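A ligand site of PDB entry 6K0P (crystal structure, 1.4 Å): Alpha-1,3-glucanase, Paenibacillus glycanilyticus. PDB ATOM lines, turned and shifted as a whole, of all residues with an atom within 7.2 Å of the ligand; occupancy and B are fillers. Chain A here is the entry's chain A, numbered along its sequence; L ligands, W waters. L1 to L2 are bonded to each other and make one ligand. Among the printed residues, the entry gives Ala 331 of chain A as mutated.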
ATOM      1  N   TYR A 122      11.682  -1.893  16.593  1.00  0.00           N
ATOM      2  CA  TYR A 122      10.598  -2.655  15.992  1.00  0.00           C
ATOM      3  C   TYR A 122      11.023  -3.979  15.375  1.00  0.00           C
ATOM      4  O   TYR A 122      10.201  -4.899  15.279  1.00  0.00           O
ATOM      5  CB  TYR A 122       9.921  -1.845  14.883  1.00  0.00           C
ATOM      6  CG  TYR A 122       8.980  -0.754  15.360  1.00  0.00           C
ATOM      7  CD1 TYR A 122       7.667  -1.037  15.710  1.00  0.00           C
ATOM      8  CD2 TYR A 122       9.418   0.566  15.449  1.00  0.00           C
ATOM      9  CE1 TYR A 122       6.805  -0.035  16.132  1.00  0.00           C
ATOM     10  CE2 TYR A 122       8.578   1.566  15.874  1.00  0.00           C
ATOM     11  CZ  TYR A 122       7.271   1.278  16.212  1.00  0.00           C
ATOM     12  OH  TYR A 122       6.448   2.296  16.617  1.00  0.00           O
ATOM     13  N   ARG A 280       9.315  -3.976  19.753  1.00  0.00           N
ATOM     14  CA  ARG A 280       8.165  -3.126  19.999  1.00  0.00           C
ATOM     15  C   ARG A 280       6.986  -3.575  19.153  1.00  0.00           C
ATOM     16  O   ARG A 280       7.147  -3.952  17.986  1.00  0.00           O
ATOM     17  CB  ARG A 280       8.537  -1.683  19.622  1.00  0.00           C
ATOM     18  CG  ARG A 280       7.441  -0.662  19.843  1.00  0.00           C
ATOM     19  CD  ARG A 280       7.995   0.735  19.580  1.00  0.00           C
ATOM     20  NE  ARG A 280       6.958   1.743  19.697  1.00  0.00           N
ATOM     21  CZ  ARG A 280       7.200   3.048  19.845  1.00  0.00           C
ATOM     22  NH1 ARG A 280       8.440   3.492  19.892  1.00  0.00           N
ATOM     23  NH2 ARG A 280       6.182   3.905  19.955  1.00  0.00           N
ATOM     24  N   VAL A 281       5.797  -3.535  19.756  1.00  0.00           N
ATOM     25  CA  VAL A 281       4.530  -3.720  19.065  1.00  0.00           C
ATOM     26  C   VAL A 281       3.601  -2.628  19.564  1.00  0.00           C
ATOM     27  O   VAL A 281       3.503  -2.401  20.770  1.00  0.00           O
ATOM     28  CB  VAL A 281       3.929  -5.113  19.347  1.00  0.00           C
ATOM     29  CG1 VAL A 281       2.653  -5.342  18.529  1.00  0.00           C
ATOM     30  CG2 VAL A 281       4.952  -6.214  19.068  1.00  0.00           C
ATOM     31  N   ASP A 282       2.923  -1.943  18.651  1.00  0.00           N
ATOM     32  CA  ASP A 282       2.088  -0.810  19.014  1.00  0.00           C
ATOM     33  C   ASP A 282       0.638  -1.266  19.147  1.00  0.00           C
ATOM     34  O   ASP A 282       0.012  -1.666  18.151  1.00  0.00           O
ATOM     35  CB  ASP A 282       2.211   0.334  18.006  1.00  0.00           C
ATOM     36  CG  ASP A 282       3.603   0.953  18.010  1.00  0.00           C
ATOM     37  OD1 ASP A 282       4.302   0.893  19.036  1.00  0.00           O
ATOM     38  OD2 ASP A 282       3.985   1.523  16.968  1.00  0.00           O
ATOM     39  N   GLY A 283       0.113  -1.172  20.354  1.00  0.00           N
ATOM     40  CA  GLY A 283      -1.211  -1.643  20.689  1.00  0.00           C
ATOM     41  C   GLY A 283      -1.151  -2.440  21.965  1.00  0.00           C
ATOM     42  O   GLY A 283      -1.382  -1.921  23.058  1.00  0.00           O
ATOM     43  N   PRO A 284      -0.808  -3.715  21.863  1.00  0.00           N
ATOM     44  CA  PRO A 284      -0.583  -4.539  23.054  1.00  0.00           C
ATOM     45  C   PRO A 284       0.754  -4.193  23.689  1.00  0.00           C
ATOM     46  O   PRO A 284       1.551  -3.447  23.144  1.00  0.00           O
ATOM     47  CB  PRO A 284      -0.544  -5.956  22.470  1.00  0.00           C
ATOM     48  CG  PRO A 284       0.010  -5.773  21.092  1.00  0.00           C
ATOM     49  CD  PRO A 284      -0.605  -4.482  20.615  1.00  0.00           C
ATOM     50  N   GLY A 285       0.989  -4.772  24.865  1.00  0.00           N
ATOM     51  CA  GLY A 285       2.319  -4.760  25.445  1.00  0.00           C
ATOM     52  C   GLY A 285       2.545  -3.889  26.656  1.00  0.00           C
ATOM     53  O   GLY A 285       3.693  -3.757  27.098  1.00  0.00           O
ATOM     54  N   LYS A 286       1.501  -3.285  27.219  1.00  0.00           N
ATOM     55  CA  LYS A 286       1.661  -2.557  28.469  1.00  0.00           C
ATOM     56  C   LYS A 286       1.457  -3.518  29.620  1.00  0.00           C
ATOM     57  O   LYS A 286       0.477  -4.278  29.625  1.00  0.00           O
ATOM     58  CB  LYS A 286       0.663  -1.398  28.556  1.00  0.00           C
ATOM     59  CG  LYS A 286       0.915  -0.297  27.533  1.00  0.00           C
ATOM     60  CD  LYS A 286       0.098  -0.477  26.264  1.00  0.00           C
ATOM     61  CE  LYS A 286       0.289   0.730  25.355  1.00  0.00           C
ATOM     62  NZ  LYS A 286      -0.547   0.635  24.118  1.00  0.00           N
ATOM     63  N   VAL A 307       6.370  -3.549  26.336  1.00  0.00           N
ATOM     64  CA  VAL A 307       6.398  -2.339  25.516  1.00  0.00           C
ATOM     65  C   VAL A 307       6.411  -1.105  26.402  1.00  0.00           C
ATOM     66  O   VAL A 307       7.249  -0.208  26.243  1.00  0.00           O
ATOM     67  CB  VAL A 307       5.260  -2.353  24.480  1.00  0.00           C
ATOM     68  CG1 VAL A 307       5.312  -1.080  23.612  1.00  0.00           C
ATOM     69  CG2 VAL A 307       5.378  -3.593  23.595  1.00  0.00           C
ATOM     70  N   CYS A 308       5.515  -1.068  27.397  1.00  0.00           N
ATOM     71  CA  CYS A 308       5.497   0.002  28.392  1.00  0.00           C
ATOM     72  C   CYS A 308       5.139  -0.580  29.745  1.00  0.00           C
ATOM     73  O   CYS A 308       4.576  -1.677  29.833  1.00  0.00           O
ATOM     74  CB  CYS A 308       4.402   1.060  28.111  1.00  0.00           C
ATOM     75  SG  CYS A 308       4.341   1.670  26.427  1.00  0.00           S
ATOM     76  N   TRP A 311       0.325   3.207  30.113  1.00  0.00           N
ATOM     77  CA  TRP A 311      -0.040   4.231  29.132  1.00  0.00           C
ATOM     78  C   TRP A 311      -1.449   4.683  29.527  1.00  0.00           C
ATOM     79  O   TRP A 311      -2.436   4.073  29.121  1.00  0.00           O
ATOM     80  CB  TRP A 311      -0.023   3.632  27.736  1.00  0.00           C
ATOM     81  CG  TRP A 311      -0.260   4.608  26.621  1.00  0.00           C
ATOM     82  CD1 TRP A 311      -1.453   5.182  26.263  1.00  0.00           C
ATOM     83  CD2 TRP A 311       0.720   5.098  25.709  1.00  0.00           C
ATOM     84  NE1 TRP A 311      -1.269   6.008  25.176  1.00  0.00           N
ATOM     85  CE2 TRP A 311       0.062   5.986  24.825  1.00  0.00           C
ATOM     86  CE3 TRP A 311       2.095   4.904  25.557  1.00  0.00           C
ATOM     87  CZ2 TRP A 311       0.726   6.654  23.805  1.00  0.00           C
ATOM     88  CZ3 TRP A 311       2.754   5.560  24.540  1.00  0.00           C
ATOM     89  CH2 TRP A 311       2.070   6.432  23.670  1.00  0.00           C
ATOM     90  N   GLY A 312      -1.508   5.756  30.313  1.00  0.00           N
ATOM     91  CA  GLY A 312      -2.786   6.216  30.832  1.00  0.00           C
ATOM     92  C   GLY A 312      -3.593   6.962  29.786  1.00  0.00           C
ATOM     93  O   GLY A 312      -3.043   7.655  28.925  1.00  0.00           O
ATOM     94  N   VAL A 313      -4.907   6.787  29.853  1.00  0.00           N
ATOM     95  CA  VAL A 313      -5.854   7.454  28.959  1.00  0.00           C
ATOM     96  C   VAL A 313      -6.975   7.988  29.854  1.00  0.00           C
ATOM     97  O   VAL A 313      -7.785   7.214  30.365  1.00  0.00           O
ATOM     98  CB  VAL A 313      -6.423   6.504  27.896  1.00  0.00           C
ATOM     99  CG1 VAL A 313      -7.350   7.268  26.976  1.00  0.00           C
ATOM    100  CG2 VAL A 313      -5.290   5.836  27.113  1.00  0.00           C
ATOM    101  N   PHE A 329      10.393  -1.691  25.347  1.00  0.00           N
ATOM    102  CA  PHE A 329      10.487  -1.482  23.905  1.00  0.00           C
ATOM    103  C   PHE A 329       9.827  -0.205  23.415  1.00  0.00           C
ATOM    104  O   PHE A 329      10.020   0.166  22.249  1.00  0.00           O
ATOM    105  CB  PHE A 329      10.019  -2.743  23.158  1.00  0.00           C
ATOM    106  CG  PHE A 329      10.990  -3.875  23.347  1.00  0.00           C
ATOM    107  CD1 PHE A 329      12.078  -4.016  22.502  1.00  0.00           C
ATOM    108  CD2 PHE A 329      10.872  -4.717  24.437  1.00  0.00           C
ATOM    109  CE1 PHE A 329      13.005  -5.023  22.707  1.00  0.00           C
ATOM    110  CE2 PHE A 329      11.801  -5.729  24.654  1.00  0.00           C
ATOM    111  CZ  PHE A 329      12.864  -5.872  23.791  1.00  0.00           C
ATOM    112  N   ALA A 330       9.107   0.493  24.288  1.00  0.00           N
ATOM    113  CA  ALA A 330       8.635   1.848  24.004  1.00  0.00           C
ATOM    114  C   ALA A 330       8.662   2.654  25.292  1.00  0.00           C
ATOM    115  O   ALA A 330       9.516   2.416  26.154  1.00  0.00           O
ATOM    116  CB  ALA A 330       7.265   1.835  23.330  1.00  0.00           C
ATOM    117  N   ALA A 331       7.722   3.586  25.449  1.00  0.00           N
ATOM    118  CA  ALA A 331       7.716   4.499  26.586  1.00  0.00           C
ATOM    119  C   ALA A 331       7.626   3.751  27.914  1.00  0.00           C
ATOM    120  O   ALA A 331       7.055   2.667  28.000  1.00  0.00           O
ATOM    121  CB  ALA A 331       6.553   5.483  26.460  1.00  0.00           C
ATOM    122  N   ASN A 334       3.510   6.807  30.290  1.00  0.00           N
ATOM    123  CA  ASN A 334       2.913   7.925  29.577  1.00  0.00           C
ATOM    124  C   ASN A 334       1.525   8.118  30.147  1.00  0.00           C
ATOM    125  O   ASN A 334       0.858   7.151  30.508  1.00  0.00           O
ATOM    126  CB  ASN A 334       2.833   7.635  28.075  1.00  0.00           C
ATOM    127  CG  ASN A 334       2.532   8.869  27.234  1.00  0.00           C
ATOM    128  OD1 ASN A 334       2.425   9.985  27.742  1.00  0.00           O
ATOM    129  ND2 ASN A 334       2.393   8.662  25.929  1.00  0.00           N
ATOM    130  N   THR A 336      -1.937  10.223  29.151  1.00  0.00           N
ATOM    131  CA  THR A 336      -2.457  10.911  27.979  1.00  0.00           C
ATOM    132  C   THR A 336      -3.927  11.292  28.161  1.00  0.00           C
ATOM    133  O   THR A 336      -4.629  10.808  29.057  1.00  0.00           O
ATOM    134  CB  THR A 336      -2.329  10.073  26.701  1.00  0.00           C
ATOM    135  OG1 THR A 336      -3.394   9.114  26.646  1.00  0.00           O
ATOM    136  CG2 THR A 336      -0.994   9.349  26.651  1.00  0.00           C
ATOM    137  N   ASN A 337      -4.376  12.183  27.274  1.00  0.00           N
ATOM    138  CA  ASN A 337      -5.806  12.337  26.958  1.00  0.00           C
ATOM    139  C   ASN A 337      -6.663  12.596  28.197  1.00  0.00           C
ATOM    140  O   ASN A 337      -7.633  11.893  28.452  1.00  0.00           O
ATOM    141  CB  ASN A 337      -6.324  11.124  26.180  1.00  0.00           C
ATOM    142  CG  ASN A 337      -5.618  10.944  24.849  1.00  0.00           C
ATOM    143  OD1 ASN A 337      -4.606  11.587  24.576  1.00  0.00           O
ATOM    144  ND2 ASN A 337      -6.168  10.063  24.008  1.00  0.00           N
ATOM    145  N   ASP A 354      11.268   4.349  24.069  1.00  0.00           N
ATOM    146  CA  ASP A 354      10.701   5.636  23.650  1.00  0.00           C
ATOM    147  C   ASP A 354      10.739   6.522  24.898  1.00  0.00           C
ATOM    148  O   ASP A 354      11.397   6.156  25.881  1.00  0.00           O
ATOM    149  CB  ASP A 354       9.307   5.442  23.044  1.00  0.00           C
ATOM    150  CG  ASP A 354       8.971   6.495  21.991  1.00  0.00           C
ATOM    151  OD1 ASP A 354       8.885   7.694  22.327  1.00  0.00           O
ATOM    152  OD2 ASP A 354       8.758   6.115  20.824  1.00  0.00           O
ATOM    153  N   PHE A 360       1.145  13.447  27.621  1.00  0.00           N
ATOM    154  CA  PHE A 360       0.594  13.906  26.350  1.00  0.00           C
ATOM    155  C   PHE A 360      -0.799  14.465  26.592  1.00  0.00           C
ATOM    156  O   PHE A 360      -1.744  13.703  26.856  1.00  0.00           O
ATOM    157  CB  PHE A 360       0.557  12.800  25.289  1.00  0.00           C
ATOM    158  CG  PHE A 360       0.254  13.330  23.903  1.00  0.00           C
ATOM    159  CD1 PHE A 360      -1.050  13.637  23.517  1.00  0.00           C
ATOM    160  CD2 PHE A 360       1.279  13.576  22.995  1.00  0.00           C
ATOM    161  CE1 PHE A 360      -1.314  14.145  22.255  1.00  0.00           C
ATOM    162  CE2 PHE A 360       1.016  14.084  21.732  1.00  0.00           C
ATOM    163  CZ  PHE A 360      -0.270  14.363  21.361  1.00  0.00           C
ATOM    164  N   ALA A 362      -4.296  16.085  25.591  1.00  0.00           N
ATOM    165  CA  ALA A 362      -5.227  16.126  24.480  1.00  0.00           C
ATOM    166  C   ALA A 362      -6.630  16.156  25.053  1.00  0.00           C
ATOM    167  O   ALA A 362      -6.839  15.790  26.210  1.00  0.00           O
ATOM    168  CB  ALA A 362      -5.048  14.914  23.547  1.00  0.00           C
ATOM    169  N   TYR A 422      -3.479  14.583  16.574  1.00  0.00           N
ATOM    170  CA  TYR A 422      -4.526  14.347  17.562  1.00  0.00           C
ATOM    171  C   TYR A 422      -5.226  15.664  17.913  1.00  0.00           C
ATOM    172  O   TYR A 422      -4.827  16.753  17.496  1.00  0.00           O
ATOM    173  CB  TYR A 422      -3.950  13.670  18.805  1.00  0.00           C
ATOM    174  CG  TYR A 422      -3.301  12.331  18.486  1.00  0.00           C
ATOM    175  CD1 TYR A 422      -4.074  11.204  18.229  1.00  0.00           C
ATOM    176  CD2 TYR A 422      -1.916  12.190  18.465  1.00  0.00           C
ATOM    177  CE1 TYR A 422      -3.487   9.981  17.950  1.00  0.00           C
ATOM    178  CE2 TYR A 422      -1.328  10.976  18.190  1.00  0.00           C
ATOM    179  CZ  TYR A 422      -2.109   9.870  17.935  1.00  0.00           C
ATOM    180  OH  TYR A 422      -1.523   8.662  17.647  1.00  0.00           O
HETATM  181  C1  LIG L   1       2.515   4.484  19.594  1.00  0.00           C
HETATM  182  C2  LIG L   1       1.013   4.272  19.614  1.00  0.00           C
HETATM  183  C3  LIG L   1       0.555   4.117  21.046  1.00  0.00           C
HETATM  184  C4  LIG L   1       1.344   3.016  21.749  1.00  0.00           C
HETATM  185  C5  LIG L   1       2.811   3.336  21.680  1.00  0.00           C
HETATM  186  C6  LIG L   1       3.697   2.216  22.213  1.00  0.00           C
HETATM  187  O1  LIG L   1       2.736   5.730  20.144  1.00  0.00           O
HETATM  188  O2  LIG L   1       0.412   5.392  18.951  1.00  0.00           O
HETATM  189  O3  LIG L   1      -0.780   3.654  21.026  1.00  0.00           O
HETATM  190  O4  LIG L   1       0.983   2.892  23.095  1.00  0.00           O
HETATM  191  O5  LIG L   1       3.179   3.510  20.345  1.00  0.00           O
HETATM  192  O6  LIG L   1       3.475   0.965  21.622  1.00  0.00           O
HETATM  193  C1  LG2 L   2      -1.646   4.294  22.030  1.00  0.00           C
HETATM  194  C2  LG2 L   2      -2.999   3.594  22.061  1.00  0.00           C
HETATM  195  C3  LG2 L   2      -3.788   4.007  20.821  1.00  0.00           C
HETATM  196  C4  LG2 L   2      -3.882   5.525  20.731  1.00  0.00           C
HETATM  197  C5  LG2 L   2      -2.484   6.137  20.802  1.00  0.00           C
HETATM  198  C6  LG2 L   2      -2.483   7.664  20.758  1.00  0.00           C
HETATM  199  O1  LG2 L   2      -2.799   2.189  22.052  1.00  0.00           O
HETATM  200  O2  LG2 L   2      -5.070   3.421  20.831  1.00  0.00           O
HETATM  201  O3  LG2 L   2      -4.506   5.890  19.514  1.00  0.00           O
HETATM  202  O4  LG2 L   2      -1.841   5.697  21.990  1.00  0.00           O
HETATM  203  O5  LG2 L   2      -3.278   8.193  21.809  1.00  0.00           O
HETATM  204  O   HOH W   1      -6.584   3.841  23.648  1.00  0.00           O
HETATM  205  O   HOH W   2      -3.492   7.563  24.295  1.00  0.00           O
HETATM  206  O   HOH W   3      -5.119   1.156  19.198  1.00  0.00           O
HETATM  207  O   HOH W   4      -6.404   8.342  20.030  1.00  0.00           O
HETATM  208  O   HOH W   5      -3.136   0.751  25.134  1.00  0.00           O
HETATM  209  O   HOH W   6       1.005   7.945  19.395  1.00  0.00           O
HETATM  210  O   HOH W   7      -3.015   6.308  17.030  1.00  0.00           O
HETATM  211  O   HOH W   8      -2.281   1.107  19.474  1.00  0.00           O
HETATM  212  O   HOH W   9       1.644  -0.688  22.685  1.00  0.00           O
HETATM  213  O   HOH W  10      -4.908   0.932  23.131  1.00  0.00           O
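Merely in contact with the ligand: Val 307 (3.4 Å), Tyr 422 (3.4 Å) and Ala 330 (3.8 Å).
Eight residues have an atom within 4 Å of the ligand: Arg 280, Val 281, Asp 282, Lys 286, Val 307, Trp 311, Ala 330 and Tyr 422.
The nearest printed residue that does not touch the ligand is Asn 337 (4.1 Å).
OD1 of Asp 282 lies within hydrogen-bond range of O6 of LIG L1, 2.7 Å away.
NZ of Lys 286 lies within hydrogen-bond range of O4 of LIG L1, 2.9 Å away.
O5 of LIG L1 is in hydrogen-bond range of NH2 of Arg 280 (3.1 Å).
NE1 of Trp 311 is in hydrogen-bond range of O4 of LG2 L2, 3.3 Å away.
An oxygen (O6) of LIG L1 sits at hydrogen-bond distance from the backbone carbonyl oxygen (O) of Val 281, 3.5 Å away.
NE of Arg 280 lies within salt-bridge range of OD1 of Asp 282.
OH of Tyr 122 lies within hydrogen-bond range of OD2 of Asp 282 (2.6 Å).
NZ of Lys 286 lies within hydrogen-bond range of O of Gly 283, at 2.9 Å.
OH of Tyr 122 is in hydrogen-bond range of NE of Arg 280 (3.2 Å).
OD2 of Asp 354 lies within salt-bridge range of NH1 of Arg 280 (2.8 Å).
The backbone NH of Ala 330 is in hydrogen-bond range of the backbone carbonyl oxygen of Val 307 (2.8 Å).
N of Val 307 lies within hydrogen-bond range of O of Gly 285.
O of Ala 330 sits at hydrogen-bond distance from N of Asp 354 (3.3 Å).
Water W2 lies within hydrogen-bond range of O5 of LG2 L2 (2.6 Å), OG1 of Thr 336 (2.8 Å) and NE1 of Trp 311 (2.9 Å).
Water W6 lies within hydrogen-bond range of an oxygen (O2) of LIG L1 (2.7 Å) and the side-chain hydroxyl (OH) of Tyr 422 (3.2 Å).
Water W9 lies within hydrogen-bond range of an oxygen (O6) of LIG L1 (2.7 Å), the backbone carbonyl oxygen of Pro 284 (2.8 Å), the backbone NH of Gly 283 (2.8 Å), the side-chain amino group of Lys 286 (2.9 Å) and the backbone carbonyl oxygen of Val 281 (3.2 Å).
Water W8 lies within hydrogen-bond range of an oxygen (O1) of LG2 L2 (2.8 Å) and the backbone NH (N) of Gly 283 (3.4 Å).
Water W7 lies within hydrogen-bond range of OH of Tyr 422 (2.9 Å) and O3 of LG2 L2 (2.9 Å).
Water W5 lies within hydrogen-bond range of the side-chain amino group of Lys 286 and an oxygen (O1) of LG2 L2.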
